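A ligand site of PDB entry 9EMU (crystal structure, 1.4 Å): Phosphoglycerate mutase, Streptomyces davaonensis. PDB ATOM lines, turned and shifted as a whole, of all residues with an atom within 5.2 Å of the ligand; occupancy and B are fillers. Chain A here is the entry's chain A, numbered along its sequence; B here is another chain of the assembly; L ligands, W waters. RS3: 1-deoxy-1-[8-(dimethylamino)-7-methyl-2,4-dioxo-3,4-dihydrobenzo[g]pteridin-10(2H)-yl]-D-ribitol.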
ATOM      1  N   ARG A  45     -24.390  31.385  14.397  1.00  0.00           N
ATOM      2  CA  ARG A  45     -24.372  30.371  13.340  1.00  0.00           C
ATOM      3  C   ARG A  45     -25.631  29.523  13.435  1.00  0.00           C
ATOM      4  O   ARG A  45     -26.100  29.202  14.526  1.00  0.00           O
ATOM      5  CB  ARG A  45     -23.135  29.483  13.426  1.00  0.00           C
ATOM      6  CG  ARG A  45     -23.058  28.512  12.250  1.00  0.00           C
ATOM      7  CD  ARG A  45     -21.828  27.629  12.333  1.00  0.00           C
ATOM      8  NE  ARG A  45     -21.812  26.692  11.212  1.00  0.00           N
ATOM      9  CZ  ARG A  45     -21.168  25.526  11.220  1.00  0.00           C
ATOM     10  NH1 ARG A  45     -20.415  25.153  12.242  1.00  0.00           N
ATOM     11  NH2 ARG A  45     -21.308  24.709  10.184  1.00  0.00           N
ATOM     12  N   TYR A  50     -26.966  18.894   8.893  1.00  0.00           N
ATOM     13  CA  TYR A  50     -26.172  17.902   8.192  1.00  0.00           C
ATOM     14  C   TYR A  50     -26.177  16.502   8.802  1.00  0.00           C
ATOM     15  O   TYR A  50     -25.648  15.581   8.172  1.00  0.00           O
ATOM     16  CB  TYR A  50     -24.713  18.396   8.067  1.00  0.00           C
ATOM     17  CG  TYR A  50     -24.615  19.847   7.662  1.00  0.00           C
ATOM     18  CD1 TYR A  50     -25.084  20.275   6.414  1.00  0.00           C
ATOM     19  CD2 TYR A  50     -24.056  20.787   8.513  1.00  0.00           C
ATOM     20  CE1 TYR A  50     -24.986  21.603   6.044  1.00  0.00           C
ATOM     21  CE2 TYR A  50     -23.951  22.110   8.147  1.00  0.00           C
ATOM     22  CZ  TYR A  50     -24.426  22.514   6.926  1.00  0.00           C
ATOM     23  OH  TYR A  50     -24.321  23.843   6.568  1.00  0.00           O
ATOM     24  N   GLU A 119     -23.567  32.171   3.079  1.00  0.00           N
ATOM     25  CA  GLU A 119     -22.259  31.582   3.273  1.00  0.00           C
ATOM     26  C   GLU A 119     -21.364  31.874   2.075  1.00  0.00           C
ATOM     27  O   GLU A 119     -21.841  32.150   0.953  1.00  0.00           O
ATOM     28  CB  GLU A 119     -22.392  30.062   3.490  1.00  0.00           C
ATOM     29  CG  GLU A 119     -21.108  29.244   3.814  1.00  0.00           C
ATOM     30  CD  GLU A 119     -20.299  29.770   5.007  1.00  0.00           C
ATOM     31  OE1 GLU A 119     -19.865  30.940   4.986  1.00  0.00           O
ATOM     32  OE2 GLU A 119     -20.097  29.018   5.988  1.00  0.00           O
ATOM     33  N   SER A 130     -15.231  19.021  -2.762  1.00  0.00           N
ATOM     34  CA  SER A 130     -14.665  19.679  -1.599  1.00  0.00           C
ATOM     35  C   SER A 130     -13.246  19.168  -1.336  1.00  0.00           C
ATOM     36  O   SER A 130     -12.921  17.999  -1.601  1.00  0.00           O
ATOM     37  CB  SER A 130     -15.552  19.439  -0.374  1.00  0.00           C
ATOM     38  OG  SER A 130     -16.859  19.959  -0.607  1.00  0.00           O
ATOM     39  N   GLU A 131     -12.403  20.043  -0.813  1.00  0.00           N
ATOM     40  CA  GLU A 131     -11.011  19.698  -0.557  1.00  0.00           C
ATOM     41  C   GLU A 131     -10.627  20.175   0.832  1.00  0.00           C
ATOM     42  O   GLU A 131     -10.955  21.296   1.226  1.00  0.00           O
ATOM     43  CB  GLU A 131     -10.071  20.384  -1.557  1.00  0.00           C
ATOM     44  CG  GLU A 131     -10.451  20.174  -3.019  1.00  0.00           C
ATOM     45  CD  GLU A 131      -9.499  20.867  -3.986  1.00  0.00           C
ATOM     46  OE1 GLU A 131      -8.553  21.543  -3.510  1.00  0.00           O
ATOM     47  OE2 GLU A 131      -9.691  20.732  -5.212  1.00  0.00           O
ATOM     48  N   LEU A 132      -9.971  19.300   1.590  1.00  0.00           N
ATOM     49  CA  LEU A 132      -9.420  19.701   2.880  1.00  0.00           C
ATOM     50  C   LEU A 132      -8.094  20.429   2.642  1.00  0.00           C
ATOM     51  O   LEU A 132      -7.155  19.858   2.071  1.00  0.00           O
ATOM     52  CB  LEU A 132      -9.182  18.478   3.758  1.00  0.00           C
ATOM     53  CG  LEU A 132      -8.567  18.743   5.121  1.00  0.00           C
ATOM     54  CD1 LEU A 132      -9.499  19.564   6.009  1.00  0.00           C
ATOM     55  CD2 LEU A 132      -8.203  17.457   5.825  1.00  0.00           C
ATOM     56  N   LYS A 133      -8.023  21.703   3.059  1.00  0.00           N
ATOM     57  CA  LYS A 133      -6.825  22.490   2.853  1.00  0.00           C
ATOM     58  C   LYS A 133      -6.004  22.535   4.132  1.00  0.00           C
ATOM     59  O   LYS A 133      -6.556  22.451   5.236  1.00  0.00           O
ATOM     60  CB  LYS A 133      -7.190  23.932   2.480  1.00  0.00           C
ATOM     61  CG  LYS A 133      -7.795  24.109   1.085  1.00  0.00           C
ATOM     62  CD  LYS A 133      -6.798  23.654   0.028  1.00  0.00           C
ATOM     63  CE  LYS A 133      -7.113  24.264  -1.328  1.00  0.00           C
ATOM     64  NZ  LYS A 133      -8.404  23.771  -1.878  1.00  0.00           N
ATOM     65  N   PRO A 139      -9.812  28.092   1.376  1.00  0.00           N
ATOM     66  CA  PRO A 139     -10.434  26.947   0.682  1.00  0.00           C
ATOM     67  C   PRO A 139     -11.602  27.298  -0.246  1.00  0.00           C
ATOM     68  O   PRO A 139     -12.204  26.360  -0.787  1.00  0.00           O
ATOM     69  CB  PRO A 139     -10.928  26.085   1.848  1.00  0.00           C
ATOM     70  CG  PRO A 139     -11.233  27.034   2.919  1.00  0.00           C
ATOM     71  CD  PRO A 139     -10.303  28.228   2.761  1.00  0.00           C
ATOM     72  N   PHE A 140     -11.925  28.561  -0.445  1.00  0.00           N
ATOM     73  CA  PHE A 140     -13.179  28.860  -1.129  1.00  0.00           C
ATOM     74  C   PHE A 140     -12.940  29.618  -2.431  1.00  0.00           C
ATOM     75  O   PHE A 140     -11.979  30.385  -2.538  1.00  0.00           O
ATOM     76  CB  PHE A 140     -14.086  29.724  -0.231  1.00  0.00           C
ATOM     77  CG  PHE A 140     -14.241  29.192   1.157  1.00  0.00           C
ATOM     78  CD1 PHE A 140     -14.874  27.974   1.385  1.00  0.00           C
ATOM     79  CD2 PHE A 140     -13.737  29.881   2.233  1.00  0.00           C
ATOM     80  CE1 PHE A 140     -14.997  27.464   2.678  1.00  0.00           C
ATOM     81  CE2 PHE A 140     -13.854  29.389   3.514  1.00  0.00           C
ATOM     82  CZ  PHE A 140     -14.474  28.189   3.743  1.00  0.00           C
ATOM     83  N   ASP A 178     -20.829  29.855   9.141  1.00  0.00           N
ATOM     84  CA  ASP A 178     -19.520  29.792   9.767  1.00  0.00           C
ATOM     85  C   ASP A 178     -18.459  30.634   9.073  1.00  0.00           C
ATOM     86  O   ASP A 178     -17.863  31.535   9.675  1.00  0.00           O
ATOM     87  CB  ASP A 178     -19.052  28.322   9.818  1.00  0.00           C
ATOM     88  CG  ASP A 178     -17.614  28.157  10.284  1.00  0.00           C
ATOM     89  OD1 ASP A 178     -17.241  28.709  11.343  1.00  0.00           O
ATOM     90  OD2 ASP A 178     -16.849  27.458   9.575  1.00  0.00           O
ATOM     91  N   SER A 179     -18.150  30.284   7.826  1.00  0.00           N
ATOM     92  CA  SER A 179     -16.968  30.897   7.228  1.00  0.00           C
ATOM     93  C   SER A 179     -17.171  32.385   6.961  1.00  0.00           C
ATOM     94  O   SER A 179     -16.242  33.180   7.172  1.00  0.00           O
ATOM     95  CB  SER A 179     -16.590  30.124   5.972  1.00  0.00           C
ATOM     96  OG  SER A 179     -16.218  28.826   6.394  1.00  0.00           O
ATOM     97  N   VAL A 182     -16.695  34.056  10.340  1.00  0.00           N
ATOM     98  CA  VAL A 182     -15.287  34.063  10.722  1.00  0.00           C
ATOM     99  C   VAL A 182     -14.510  35.087   9.900  1.00  0.00           C
ATOM    100  O   VAL A 182     -13.647  35.802  10.426  1.00  0.00           O
ATOM    101  CB  VAL A 182     -14.680  32.654  10.589  1.00  0.00           C
ATOM    102  CG1 VAL A 182     -13.150  32.693  10.622  1.00  0.00           C
ATOM    103  CG2 VAL A 182     -15.237  31.753  11.653  1.00  0.00           C
ATOM    104  N   TRP A 193      -7.662  35.143   6.599  1.00  0.00           N
ATOM    105  CA  TRP A 193      -8.069  33.763   6.826  1.00  0.00           C
ATOM    106  C   TRP A 193      -6.924  32.942   7.380  1.00  0.00           C
ATOM    107  O   TRP A 193      -5.804  32.940   6.853  1.00  0.00           O
ATOM    108  CB  TRP A 193      -8.582  33.146   5.531  1.00  0.00           C
ATOM    109  CG  TRP A 193      -9.077  31.743   5.717  1.00  0.00           C
ATOM    110  CD1 TRP A 193      -8.361  30.598   5.537  1.00  0.00           C
ATOM    111  CD2 TRP A 193     -10.373  31.338   6.138  1.00  0.00           C
ATOM    112  NE1 TRP A 193      -9.147  29.494   5.817  1.00  0.00           N
ATOM    113  CE2 TRP A 193     -10.392  29.929   6.183  1.00  0.00           C
ATOM    114  CE3 TRP A 193     -11.545  32.040   6.476  1.00  0.00           C
ATOM    115  CZ2 TRP A 193     -11.512  29.208   6.569  1.00  0.00           C
ATOM    116  CZ3 TRP A 193     -12.671  31.307   6.857  1.00  0.00           C
ATOM    117  CH2 TRP A 193     -12.641  29.901   6.893  1.00  0.00           C
ATOM    118  N   ASP A 197      -8.084  31.456  13.959  1.00  0.00           N
ATOM    119  CA  ASP A 197      -8.122  30.064  13.505  1.00  0.00           C
ATOM    120  C   ASP A 197      -9.168  29.302  14.315  1.00  0.00           C
ATOM    121  O   ASP A 197      -8.853  28.583  15.261  1.00  0.00           O
ATOM    122  CB  ASP A 197      -6.745  29.435  13.649  1.00  0.00           C
ATOM    123  CG  ASP A 197      -6.680  28.029  13.118  1.00  0.00           C
ATOM    124  OD1 ASP A 197      -7.499  27.718  12.226  1.00  0.00           O
ATOM    125  OD2 ASP A 197      -5.825  27.250  13.589  1.00  0.00           O
ATOM    126  N   MET A 198     -10.439  29.457  13.922  1.00  0.00           N
ATOM    127  CA  MET A 198     -11.558  28.939  14.693  1.00  0.00           C
ATOM    128  C   MET A 198     -12.655  28.484  13.749  1.00  0.00           C
ATOM    129  O   MET A 198     -12.876  29.074  12.695  1.00  0.00           O
ATOM    130  CB  MET A 198     -12.129  30.026  15.619  1.00  0.00           C
ATOM    131  CG  MET A 198     -11.148  30.540  16.644  1.00  0.00           C
ATOM    132  SD  MET A 198     -11.800  31.880  17.645  1.00  0.00           S
ATOM    133  CE  MET A 198     -13.055  31.001  18.573  1.00  0.00           C
ATOM    134  N   ILE A 199     -13.359  27.426  14.152  1.00  0.00           N
ATOM    135  CA  ILE A 199     -14.619  27.040  13.545  1.00  0.00           C
ATOM    136  C   ILE A 199     -15.739  27.394  14.524  1.00  0.00           C
ATOM    137  O   ILE A 199     -15.682  27.015  15.697  1.00  0.00           O
ATOM    138  CB  ILE A 199     -14.611  25.553  13.149  1.00  0.00           C
ATOM    139  CG1 ILE A 199     -15.933  25.169  12.485  1.00  0.00           C
ATOM    140  CG2 ILE A 199     -14.279  24.657  14.337  1.00  0.00           C
ATOM    141  CD1 ILE A 199     -15.815  23.899  11.685  1.00  0.00           C
ATOM    142  N   LEU A 200     -16.705  28.141  14.063  1.00  0.00           N
ATOM    143  CA  LEU A 200     -17.790  28.557  14.943  1.00  0.00           C
ATOM    144  C   LEU A 200     -18.766  27.399  15.132  1.00  0.00           C
ATOM    145  O   LEU A 200     -19.249  26.844  14.137  1.00  0.00           O
ATOM    146  CB  LEU A 200     -18.530  29.759  14.355  1.00  0.00           C
ATOM    147  CG  LEU A 200     -17.658  31.001  14.147  1.00  0.00           C
ATOM    148  CD1 LEU A 200     -18.473  32.105  13.496  1.00  0.00           C
ATOM    149  CD2 LEU A 200     -17.009  31.495  15.455  1.00  0.00           C
ATOM    150  N   PHE B  20     -18.545  16.852   0.638  1.00  0.00           N
ATOM    151  CA  PHE B  20     -18.713  17.983   1.539  1.00  0.00           C
ATOM    152  C   PHE B  20     -18.719  17.514   2.985  1.00  0.00           C
ATOM    153  O   PHE B  20     -18.024  18.077   3.839  1.00  0.00           O
ATOM    154  CB  PHE B  20     -20.003  18.720   1.173  1.00  0.00           C
ATOM    155  CG  PHE B  20     -20.274  19.902   2.054  1.00  0.00           C
ATOM    156  CD1 PHE B  20     -19.640  21.102   1.825  1.00  0.00           C
ATOM    157  CD2 PHE B  20     -21.126  19.783   3.115  1.00  0.00           C
ATOM    158  CE1 PHE B  20     -19.880  22.200   2.645  1.00  0.00           C
ATOM    159  CE2 PHE B  20     -21.361  20.875   3.963  1.00  0.00           C
ATOM    160  CZ  PHE B  20     -20.733  22.075   3.722  1.00  0.00           C
ATOM    161  N   VAL B  23     -15.157  16.254   4.170  1.00  0.00           N
ATOM    162  CA  VAL B  23     -14.247  17.359   4.422  1.00  0.00           C
ATOM    163  C   VAL B  23     -14.653  18.118   5.685  1.00  0.00           C
ATOM    164  O   VAL B  23     -13.805  18.462   6.521  1.00  0.00           O
ATOM    165  CB  VAL B  23     -14.117  18.275   3.196  1.00  0.00           C
ATOM    166  CG1 VAL B  23     -13.379  19.567   3.595  1.00  0.00           C
ATOM    167  CG2 VAL B  23     -13.354  17.565   2.106  1.00  0.00           C
ATOM    168  N   MET B  24     -15.959  18.354   5.864  1.00  0.00           N
ATOM    169  CA  MET B  24     -16.431  18.987   7.084  1.00  0.00           C
ATOM    170  C   MET B  24     -16.017  18.184   8.315  1.00  0.00           C
ATOM    171  O   MET B  24     -15.571  18.753   9.320  1.00  0.00           O
ATOM    172  CB  MET B  24     -17.967  19.150   7.010  1.00  0.00           C
ATOM    173  CG  MET B  24     -18.635  19.610   8.303  1.00  0.00           C
ATOM    174  SD  MET B  24     -19.148  18.238   9.364  1.00  0.00           S
ATOM    175  CE  MET B  24     -20.322  17.390   8.327  1.00  0.00           C
ATOM    176  N   VAL B  27     -12.346  18.789   8.960  1.00  0.00           N
ATOM    177  CA  VAL B  27     -12.124  20.118   9.536  1.00  0.00           C
ATOM    178  C   VAL B  27     -12.473  20.108  11.011  1.00  0.00           C
ATOM    179  O   VAL B  27     -11.690  20.545  11.863  1.00  0.00           O
ATOM    180  CB  VAL B  27     -12.915  21.185   8.755  1.00  0.00           C
ATOM    181  CG1 VAL B  27     -12.835  22.542   9.443  1.00  0.00           C
ATOM    182  CG2 VAL B  27     -12.357  21.292   7.344  1.00  0.00           C
ATOM    183  N   TYR B  28     -13.648  19.575  11.350  1.00  0.00           N
ATOM    184  CA  TYR B  28     -14.044  19.493  12.748  1.00  0.00           C
ATOM    185  C   TYR B  28     -13.005  18.745  13.592  1.00  0.00           C
ATOM    186  O   TYR B  28     -12.639  19.198  14.681  1.00  0.00           O
ATOM    187  CB  TYR B  28     -15.410  18.815  12.861  1.00  0.00           C
ATOM    188  CG  TYR B  28     -16.582  19.760  12.803  1.00  0.00           C
ATOM    189  CD1 TYR B  28     -16.673  20.834  13.666  1.00  0.00           C
ATOM    190  CD2 TYR B  28     -17.601  19.549  11.908  1.00  0.00           C
ATOM    191  CE1 TYR B  28     -17.761  21.693  13.614  1.00  0.00           C
ATOM    192  CE2 TYR B  28     -18.701  20.401  11.848  1.00  0.00           C
ATOM    193  CZ  TYR B  28     -18.770  21.465  12.707  1.00  0.00           C
ATOM    194  OH  TYR B  28     -19.860  22.335  12.672  1.00  0.00           O
ATOM    195  N   TYR B  31     -10.055  20.604  14.901  1.00  0.00           N
ATOM    196  CA  TYR B  31     -10.378  21.505  15.991  1.00  0.00           C
ATOM    197  C   TYR B  31     -10.974  20.756  17.166  1.00  0.00           C
ATOM    198  O   TYR B  31     -11.618  21.358  18.038  1.00  0.00           O
ATOM    199  CB  TYR B  31     -11.260  22.654  15.485  1.00  0.00           C
ATOM    200  CG  TYR B  31     -10.497  23.455  14.437  1.00  0.00           C
ATOM    201  CD1 TYR B  31     -10.553  23.106  13.091  1.00  0.00           C
ATOM    202  CD2 TYR B  31      -9.638  24.490  14.805  1.00  0.00           C
ATOM    203  CE1 TYR B  31      -9.807  23.783  12.150  1.00  0.00           C
ATOM    204  CE2 TYR B  31      -8.885  25.179  13.844  1.00  0.00           C
ATOM    205  CZ  TYR B  31      -8.976  24.816  12.517  1.00  0.00           C
ATOM    206  OH  TYR B  31      -8.240  25.457  11.550  1.00  0.00           O
HETATM  207  O4  RS3 L   1     -10.019  23.041   4.383  1.00  0.00           O
HETATM  208  C4  RS3 L   1     -11.372  23.353   4.251  1.00  0.00           C
HETATM  209  N3  RS3 L   1     -12.083  22.925   3.219  1.00  0.00           N
HETATM  210  C2  RS3 L   1     -13.387  23.234   3.118  1.00  0.00           C
HETATM  211  O2  RS3 L   1     -14.074  22.773   2.075  1.00  0.00           O
HETATM  212  C4A RS3 L   1     -11.975  24.164   5.264  1.00  0.00           C
HETATM  213  C10 RS3 L   1     -13.309  24.420   5.123  1.00  0.00           C
HETATM  214  N1  RS3 L   1     -14.001  23.959   4.043  1.00  0.00           N
HETATM  215  N5  RS3 L   1     -11.248  24.604   6.374  1.00  0.00           N
HETATM  216  C5A RS3 L   1     -11.892  25.332   7.330  1.00  0.00           C
HETATM  217  C6  RS3 L   1     -11.137  25.896   8.408  1.00  0.00           C
HETATM  218  C7  RS3 L   1     -11.790  26.605   9.424  1.00  0.00           C
HETATM  219  C7M RS3 L   1     -11.010  27.128  10.641  1.00  0.00           C
HETATM  220  C8  RS3 L   1     -13.129  26.977   9.204  1.00  0.00           C
HETATM  221  N8  RS3 L   1     -13.820  27.834  10.189  1.00  0.00           N
HETATM  222  C9  RS3 L   1     -13.848  26.526   8.090  1.00  0.00           C
HETATM  223  C9A RS3 L   1     -13.237  25.657   7.154  1.00  0.00           C
HETATM  224  N10 RS3 L   1     -13.960  25.141   6.083  1.00  0.00           N
HETATM  225  C1' RS3 L   1     -15.380  25.210   5.976  1.00  0.00           C
HETATM  226  C2' RS3 L   1     -15.890  24.066   6.894  1.00  0.00           C
HETATM  227  O2' RS3 L   1     -15.263  22.800   6.556  1.00  0.00           O
HETATM  228  C3' RS3 L   1     -17.411  23.830   6.862  1.00  0.00           C
HETATM  229  O3' RS3 L   1     -18.000  24.105   5.559  1.00  0.00           O
HETATM  230  C4' RS3 L   1     -18.072  24.705   7.934  1.00  0.00           C
HETATM  231  O4' RS3 L   1     -17.810  24.179   9.229  1.00  0.00           O
HETATM  232  C5' RS3 L   1     -19.582  24.665   7.661  1.00  0.00           C
HETATM  233  O5' RS3 L   1     -19.894  23.463   6.977  1.00  0.00           O
HETATM  234  O   HOH W   1     -13.463  22.694  -0.526  1.00  0.00           O
HETATM  235  O   HOH W   2     -16.217  24.255   1.286  1.00  0.00           O
HETATM  236  O   HOH W   3     -10.610  30.227   9.682  1.00  0.00           O
HETATM  237  O   HOH W   4      -8.225  28.915   9.787  1.00  0.00           O
HETATM  238  O   HOH W   5      -8.472  24.272   6.484  1.00  0.00           O
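N8 of the ligand lies close to O of Met 198, 3.0 Å away. Residues that only touch the ligand: Arg 45, Ile 199, Tyr 31 of chain B, Val 27 of chain B, Val 23 of chain B, Pro 139, Phe 20 of chain B, Leu 132, Ser 179, Trp 193, Phe 140 and Asp 197. Hydrophobic or aromatic side chains that line the ligand: Leu 132, Pro 139, Phe 140, Trp 193, Ile 199, Phe 20 of chain B, Val 23 of chain B, Val 27 of chain B and Tyr 31 of chain B. 16 residues have an atom within 4 Å of the ligand: Arg 45, Glu 131, Leu 132, Lys 133, Pro 139, Phe 140, Asp 178, Ser 179, Trp 193, Asp 197, Met 198, Ile 199, Phe 20 of chain B, Val 23 of chain B, Val 27 of chain B and Tyr 31 of chain B.
NZ of Lys 133 is in salt-bridge range of OE1 of Glu 131, at 2.8 Å. The side-chain hydroxyl (OH) of Tyr 28 of chain B lies within hydrogen-bond range of the guanidinium group (NH1) of Arg 45. The guanidinium group of Arg 45 lies within hydrogen-bond range of the backbone carbonyl oxygen of Leu 200, at 2.8 Å. OE2 of Glu 119 sits at hydrogen-bond distance from N of Asp 178 (3.3 Å). The side-chain carboxylate (OD1) of Asp 178 lies within hydrogen-bond range of the backbone NH (N) of Leu 200 (2.8 Å). OH of Tyr 31 of chain B is in hydrogen-bond range of OD1 of Asp 197. The backbone NH (N) of Ser 179 sits at hydrogen-bond distance from the side-chain carboxylate (OE2) of Glu 119, 3.0 Å away.
Water W1 bridges O2 of the ligand and N of Glu 131. Water W5 lies within hydrogen-bond range of a nitrogen (N5) of the ligand and the backbone carbonyl oxygen (O) of Lys 133.
An oxygen (O4) of the ligand is in hydrogen-bond range of the backbone NH of Lys 133 (2.7 Å). The backbone carbonyl oxygen (O) of Glu 131 lies within hydrogen-bond range of a nitrogen (N3) of the ligand, 2.8 Å away. O4' of the ligand sits close to OD2 of Asp 178 (3.4 Å).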
